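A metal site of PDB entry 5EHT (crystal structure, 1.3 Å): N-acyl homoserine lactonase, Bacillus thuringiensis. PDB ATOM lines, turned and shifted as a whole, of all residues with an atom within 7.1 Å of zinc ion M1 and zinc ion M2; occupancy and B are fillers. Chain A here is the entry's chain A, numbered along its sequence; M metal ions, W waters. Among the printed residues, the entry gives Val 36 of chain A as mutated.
Zinc ion M1 is bound by NE2 of His 112, OD2 of Asp 194, water W1, NE2 of His 238 and OD2 of Asp 111. Zinc ion M1 has five donor atoms within binding distance.
Of the 21 residues printed, 4 come within 4 Å of zinc ion M1.
Of the 21 residues printed, 4 come within 4 Å of zinc ion M2.
A ring nitrogen (ND1) of His 112 lies within hydrogen-bond range of the side-chain carboxylate of Asp 53, 2.8 Å away. ND1 of His 112 lies within hydrogen-bond range of OG of Ser 106. N of His 238 is in hydrogen-bond range of O of Tyr 197. A ring nitrogen (ND1) of His 172 is in hydrogen-bond range of the backbone carbonyl oxygen (O) of Ala 209 (2.9 Å). ND1 of His 238 lies within hydrogen-bond range of O of Pro 37. A ring nitrogen (NE2) of His 176 sits at hydrogen-bond distance from the backbone NH (N) of Asp 194. OG of Ser 106 is in hydrogen-bond range of ND1 of His 107, 2.9 Å away.
Zinc ion M2 is bound by water W1, a ring nitrogen (NE2) of His 172, a ring nitrogen (NE2) of His 107, a ring nitrogen (ND1) of His 109 and the side-chain carboxylate (OD2) of Asp 194. Zinc ion M2 has five donor atoms within binding distance.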
ATOM      1  N   LEU A  19       2.876  -3.094  13.905  1.00  0.00           N
ATOM      2  CA  LEU A  19       3.776  -4.206  13.724  1.00  0.00           C
ATOM      3  C   LEU A  19       4.844  -3.800  12.702  1.00  0.00           C
ATOM      4  O   LEU A  19       4.526  -3.263  11.648  1.00  0.00           O
ATOM      5  CB  LEU A  19       3.108  -5.488  13.195  1.00  0.00           C
ATOM      6  CG  LEU A  19       2.096  -6.149  14.131  1.00  0.00           C
ATOM      7  CD1 LEU A  19       1.466  -7.334  13.394  1.00  0.00           C
ATOM      8  CD2 LEU A  19       2.712  -6.497  15.488  1.00  0.00           C
ATOM      9  N   VAL A  36      -1.974  -2.273  12.058  1.00  0.00           N
ATOM     10  CA  VAL A  36      -2.823  -3.389  11.659  1.00  0.00           C
ATOM     11  C   VAL A  36      -4.038  -3.445  12.600  1.00  0.00           C
ATOM     12  O   VAL A  36      -4.028  -3.048  13.754  1.00  0.00           O
ATOM     13  CB  VAL A  36      -2.106  -4.740  11.653  1.00  0.00           C
ATOM     14  CG1 VAL A  36      -0.876  -4.729  10.767  1.00  0.00           C
ATOM     15  CG2 VAL A  36      -1.784  -5.251  13.033  1.00  0.00           C
ATOM     16  N   PRO A  37      -5.169  -3.996  12.053  1.00  0.00           N
ATOM     17  CA  PRO A  37      -6.347  -4.135  12.871  1.00  0.00           C
ATOM     18  C   PRO A  37      -6.207  -5.238  13.902  1.00  0.00           C
ATOM     19  O   PRO A  37      -5.541  -6.240  13.648  1.00  0.00           O
ATOM     20  CB  PRO A  37      -7.474  -4.521  11.931  1.00  0.00           C
ATOM     21  CG  PRO A  37      -6.733  -5.168  10.806  1.00  0.00           C
ATOM     22  CD  PRO A  37      -5.414  -4.424  10.682  1.00  0.00           C
ATOM     23  N   VAL A  38      -6.794  -5.060  15.077  1.00  0.00           N
ATOM     24  CA  VAL A  38      -7.030  -6.112  16.010  1.00  0.00           C
ATOM     25  C   VAL A  38      -8.502  -6.376  16.019  1.00  0.00           C
ATOM     26  O   VAL A  38      -9.335  -5.449  16.106  1.00  0.00           O
ATOM     27  CB  VAL A  38      -6.467  -5.735  17.401  1.00  0.00           C
ATOM     28  CG1 VAL A  38      -6.919  -6.749  18.483  1.00  0.00           C
ATOM     29  CG2 VAL A  38      -4.994  -5.524  17.362  1.00  0.00           C
ATOM     30  N   ASP A  53     -11.997 -14.307  20.677  1.00  0.00           N
ATOM     31  CA  ASP A  53     -10.924 -13.458  21.157  1.00  0.00           C
ATOM     32  C   ASP A  53     -11.455 -12.233  21.927  1.00  0.00           C
ATOM     33  O   ASP A  53     -12.597 -11.894  21.915  1.00  0.00           O
ATOM     34  CB  ASP A  53      -9.984 -13.099  19.994  1.00  0.00           C
ATOM     35  CG  ASP A  53      -9.185 -14.340  19.482  1.00  0.00           C
ATOM     36  OD1 ASP A  53      -9.109 -15.320  20.247  1.00  0.00           O
ATOM     37  OD2 ASP A  53      -8.641 -14.240  18.361  1.00  0.00           O
ATOM     38  N   SER A 106      -8.468 -18.050  19.934  1.00  0.00           N
ATOM     39  CA  SER A 106      -7.720 -18.570  18.777  1.00  0.00           C
ATOM     40  C   SER A 106      -6.361 -18.954  19.220  1.00  0.00           C
ATOM     41  O   SER A 106      -5.776 -19.960  18.783  1.00  0.00           O
ATOM     42  CB  SER A 106      -7.677 -17.541  17.679  1.00  0.00           C
ATOM     43  OG  SER A 106      -6.950 -16.371  18.118  1.00  0.00           O
ATOM     44  N   HIS A 107      -5.732 -18.148  20.070  1.00  0.00           N
ATOM     45  CA  HIS A 107      -4.455 -18.364  20.662  1.00  0.00           C
ATOM     46  C   HIS A 107      -4.280 -17.304  21.796  1.00  0.00           C
ATOM     47  O   HIS A 107      -5.174 -16.465  21.968  1.00  0.00           O
ATOM     48  CB  HIS A 107      -3.340 -18.301  19.604  1.00  0.00           C
ATOM     49  CG  HIS A 107      -3.118 -17.026  18.908  1.00  0.00           C
ATOM     50  ND1 HIS A 107      -4.093 -16.361  18.186  1.00  0.00           N
ATOM     51  CD2 HIS A 107      -1.960 -16.360  18.653  1.00  0.00           C
ATOM     52  CE1 HIS A 107      -3.550 -15.372  17.520  1.00  0.00           C
ATOM     53  NE2 HIS A 107      -2.272 -15.322  17.803  1.00  0.00           N
ATOM     54  N   LEU A 108      -3.183 -17.420  22.504  1.00  0.00           N
ATOM     55  CA  LEU A 108      -3.033 -16.645  23.728  1.00  0.00           C
ATOM     56  C   LEU A 108      -2.056 -15.465  23.596  1.00  0.00           C
ATOM     57  O   LEU A 108      -1.611 -14.908  24.586  1.00  0.00           O
ATOM     58  CB  LEU A 108      -2.727 -17.518  24.923  1.00  0.00           C
ATOM     59  CG  LEU A 108      -3.830 -18.531  25.308  1.00  0.00           C
ATOM     60  CD1 LEU A 108      -3.352 -19.468  26.391  1.00  0.00           C
ATOM     61  CD2 LEU A 108      -5.171 -17.858  25.618  1.00  0.00           C
ATOM     62  N   HIS A 109      -1.695 -15.040  22.398  1.00  0.00           N
ATOM     63  CA  HIS A 109      -0.993 -13.807  22.189  1.00  0.00           C
ATOM     64  C   HIS A 109      -1.778 -12.640  22.762  1.00  0.00           C
ATOM     65  O   HIS A 109      -3.034 -12.693  22.856  1.00  0.00           O
ATOM     66  CB  HIS A 109      -0.726 -13.544  20.702  1.00  0.00           C
ATOM     67  CG  HIS A 109       0.318 -14.447  20.141  1.00  0.00           C
ATOM     68  ND1 HIS A 109       0.545 -14.536  18.801  1.00  0.00           N
ATOM     69  CD2 HIS A 109       1.160 -15.305  20.749  1.00  0.00           C
ATOM     70  CE1 HIS A 109       1.536 -15.398  18.602  1.00  0.00           C
ATOM     71  NE2 HIS A 109       1.919 -15.880  19.759  1.00  0.00           N
ATOM     72  N   PHE A 110      -1.057 -11.608  23.150  1.00  0.00           N
ATOM     73  CA  PHE A 110      -1.650 -10.505  23.935  1.00  0.00           C
ATOM     74  C   PHE A 110      -2.766  -9.780  23.214  1.00  0.00           C
ATOM     75  O   PHE A 110      -3.645  -9.214  23.883  1.00  0.00           O
ATOM     76  CB  PHE A 110      -0.567  -9.512  24.426  1.00  0.00           C
ATOM     77  CG  PHE A 110      -0.188  -8.486  23.417  1.00  0.00           C
ATOM     78  CD1 PHE A 110       0.503  -8.780  22.251  1.00  0.00           C
ATOM     79  CD2 PHE A 110      -0.605  -7.242  23.598  1.00  0.00           C
ATOM     80  CE1 PHE A 110       0.741  -7.773  21.295  1.00  0.00           C
ATOM     81  CE2 PHE A 110      -0.333  -6.251  22.708  1.00  0.00           C
ATOM     82  CZ  PHE A 110       0.324  -6.503  21.541  1.00  0.00           C
ATOM     83  N   ASP A 111      -2.738  -9.775  21.867  1.00  0.00           N
ATOM     84  CA  ASP A 111      -3.738  -9.114  21.087  1.00  0.00           C
ATOM     85  C   ASP A 111      -4.988  -9.989  20.852  1.00  0.00           C
ATOM     86  O   ASP A 111      -5.927  -9.494  20.231  1.00  0.00           O
ATOM     87  CB  ASP A 111      -3.142  -8.572  19.753  1.00  0.00           C
ATOM     88  CG  ASP A 111      -2.491  -9.670  18.874  1.00  0.00           C
ATOM     89  OD1 ASP A 111      -1.684 -10.474  19.463  1.00  0.00           O
ATOM     90  OD2 ASP A 111      -2.748  -9.741  17.600  1.00  0.00           O
ATOM     91  N   HIS A 112      -5.014 -11.190  21.403  1.00  0.00           N
ATOM     92  CA  HIS A 112      -6.135 -12.101  21.284  1.00  0.00           C
ATOM     93  C   HIS A 112      -6.701 -12.530  22.603  1.00  0.00           C
ATOM     94  O   HIS A 112      -7.897 -12.915  22.646  1.00  0.00           O
ATOM     95  CB  HIS A 112      -5.691 -13.376  20.488  1.00  0.00           C
ATOM     96  CG  HIS A 112      -5.273 -13.010  19.100  1.00  0.00           C
ATOM     97  ND1 HIS A 112      -6.119 -13.065  18.036  1.00  0.00           N
ATOM     98  CD2 HIS A 112      -4.128 -12.441  18.629  1.00  0.00           C
ATOM     99  CE1 HIS A 112      -5.508 -12.564  16.964  1.00  0.00           C
ATOM    100  NE2 HIS A 112      -4.288 -12.174  17.304  1.00  0.00           N
ATOM    101  N   HIS A 172       1.854 -20.425  13.750  1.00  0.00           N
ATOM    102  CA  HIS A 172       1.992 -19.048  14.219  1.00  0.00           C
ATOM    103  C   HIS A 172       2.197 -19.032  15.746  1.00  0.00           C
ATOM    104  O   HIS A 172       3.050 -18.271  16.260  1.00  0.00           O
ATOM    105  CB  HIS A 172       0.771 -18.269  13.877  1.00  0.00           C
ATOM    106  CG  HIS A 172       0.735 -16.899  14.532  1.00  0.00           C
ATOM    107  ND1 HIS A 172       1.577 -15.853  14.191  1.00  0.00           N
ATOM    108  CD2 HIS A 172      -0.083 -16.426  15.478  1.00  0.00           C
ATOM    109  CE1 HIS A 172       1.274 -14.801  14.985  1.00  0.00           C
ATOM    110  NE2 HIS A 172       0.285 -15.108  15.742  1.00  0.00           N
ATOM    111  N   SER A 173       1.454 -19.888  16.454  1.00  0.00           N
ATOM    112  CA  SER A 173       1.664 -20.150  17.866  1.00  0.00           C
ATOM    113  C   SER A 173       1.529 -21.693  18.034  1.00  0.00           C
ATOM    114  O   SER A 173       0.969 -22.348  17.130  1.00  0.00           O
ATOM    115  CB  SER A 173       0.673 -19.369  18.773  1.00  0.00           C
ATOM    116  OG  SER A 173      -0.622 -19.891  18.610  1.00  0.00           O
ATOM    117  N   HIS A 176      -2.387 -22.606  17.913  1.00  0.00           N
ATOM    118  CA  HIS A 176      -3.288 -21.741  17.205  1.00  0.00           C
ATOM    119  C   HIS A 176      -4.438 -22.488  16.568  1.00  0.00           C
ATOM    120  O   HIS A 176      -4.192 -23.589  16.021  1.00  0.00           O
ATOM    121  CB  HIS A 176      -2.485 -20.967  16.125  1.00  0.00           C
ATOM    122  CG  HIS A 176      -3.309 -19.992  15.381  1.00  0.00           C
ATOM    123  ND1 HIS A 176      -4.130 -20.283  14.325  1.00  0.00           N
ATOM    124  CD2 HIS A 176      -3.501 -18.661  15.612  1.00  0.00           C
ATOM    125  CE1 HIS A 176      -4.814 -19.199  13.986  1.00  0.00           C
ATOM    126  NE2 HIS A 176      -4.421 -18.180  14.747  1.00  0.00           N
ATOM    127  N   ILE A 193      -7.804 -16.320  11.324  1.00  0.00           N
ATOM    128  CA  ILE A 193      -7.099 -15.698  12.453  1.00  0.00           C
ATOM    129  C   ILE A 193      -5.640 -15.580  11.997  1.00  0.00           C
ATOM    130  O   ILE A 193      -5.366 -15.163  10.851  1.00  0.00           O
ATOM    131  CB  ILE A 193      -7.364 -16.314  13.823  1.00  0.00           C
ATOM    132  CG1 ILE A 193      -8.811 -16.799  14.000  1.00  0.00           C
ATOM    133  CG2 ILE A 193      -6.965 -15.294  14.875  1.00  0.00           C
ATOM    134  CD1 ILE A 193      -9.886 -15.713  14.001  1.00  0.00           C
ATOM    135  N   ASP A 194      -4.702 -15.906  12.874  1.00  0.00           N
ATOM    136  CA  ASP A 194      -3.275 -15.649  12.584  1.00  0.00           C
ATOM    137  C   ASP A 194      -2.567 -16.852  11.917  1.00  0.00           C
ATOM    138  O   ASP A 194      -1.331 -16.863  11.841  1.00  0.00           O
ATOM    139  CB  ASP A 194      -2.520 -15.118  13.794  1.00  0.00           C
ATOM    140  CG  ASP A 194      -2.937 -13.697  14.238  1.00  0.00           C
ATOM    141  OD1 ASP A 194      -3.861 -13.176  13.614  1.00  0.00           O
ATOM    142  OD2 ASP A 194      -2.332 -13.295  15.284  1.00  0.00           O
ATOM    143  N   TYR A 197      -1.596 -13.735   8.496  1.00  0.00           N
ATOM    144  CA  TYR A 197      -1.903 -12.296   8.792  1.00  0.00           C
ATOM    145  C   TYR A 197      -2.574 -11.659   7.622  1.00  0.00           C
ATOM    146  O   TYR A 197      -3.496 -10.851   7.788  1.00  0.00           O
ATOM    147  CB  TYR A 197      -0.606 -11.546   9.053  1.00  0.00           C
ATOM    148  CG  TYR A 197       0.058 -11.748  10.381  1.00  0.00           C
ATOM    149  CD1 TYR A 197      -0.514 -12.353  11.502  1.00  0.00           C
ATOM    150  CD2 TYR A 197       1.300 -11.295  10.509  1.00  0.00           C
ATOM    151  CE1 TYR A 197       0.132 -12.381  12.722  1.00  0.00           C
ATOM    152  CE2 TYR A 197       1.946 -11.316  11.735  1.00  0.00           C
ATOM    153  CZ  TYR A 197       1.367 -11.813  12.832  1.00  0.00           C
ATOM    154  OH  TYR A 197       1.999 -11.802  14.020  1.00  0.00           O
ATOM    155  N   ALA A 209       5.380 -13.770  10.860  1.00  0.00           N
ATOM    156  CA  ALA A 209       5.851 -14.044  12.216  1.00  0.00           C
ATOM    157  C   ALA A 209       5.155 -15.310  12.745  1.00  0.00           C
ATOM    158  O   ALA A 209       3.936 -15.458  12.633  1.00  0.00           O
ATOM    159  CB  ALA A 209       5.541 -12.908  13.099  1.00  0.00           C
ATOM    160  N   GLY A 237      -6.073 -12.433   9.424  1.00  0.00           N
ATOM    161  CA  GLY A 237      -5.935 -11.957  10.790  1.00  0.00           C
ATOM    162  C   GLY A 237      -5.618 -10.473  10.991  1.00  0.00           C
ATOM    163  O   GLY A 237      -6.132  -9.848  11.929  1.00  0.00           O
ATOM    164  N   HIS A 238      -4.678  -9.945  10.215  1.00  0.00           N
ATOM    165  CA  HIS A 238      -4.140  -8.607  10.439  1.00  0.00           C
ATOM    166  C   HIS A 238      -3.823  -7.980   9.116  1.00  0.00           C
ATOM    167  O   HIS A 238      -2.653  -7.728   8.805  1.00  0.00           O
ATOM    168  CB  HIS A 238      -2.913  -8.665  11.371  1.00  0.00           C
ATOM    169  CG  HIS A 238      -3.109  -9.119  12.770  1.00  0.00           C
ATOM    170  ND1 HIS A 238      -3.855  -8.447  13.699  1.00  0.00           N
ATOM    171  CD2 HIS A 238      -2.602 -10.182  13.408  1.00  0.00           C
ATOM    172  CE1 HIS A 238      -3.754  -9.059  14.852  1.00  0.00           C
ATOM    173  NE2 HIS A 238      -2.995 -10.124  14.688  1.00  0.00           N
HETATM  174 ZN    ZN M   1      -2.691 -11.491  16.224  1.00  0.00          ZN
HETATM  175 ZN    ZN M   2      -0.738 -14.028  17.166  1.00  0.00          ZN
HETATM  176  O   HOH W   1      -0.929 -12.059  17.146  1.00  0.00           O
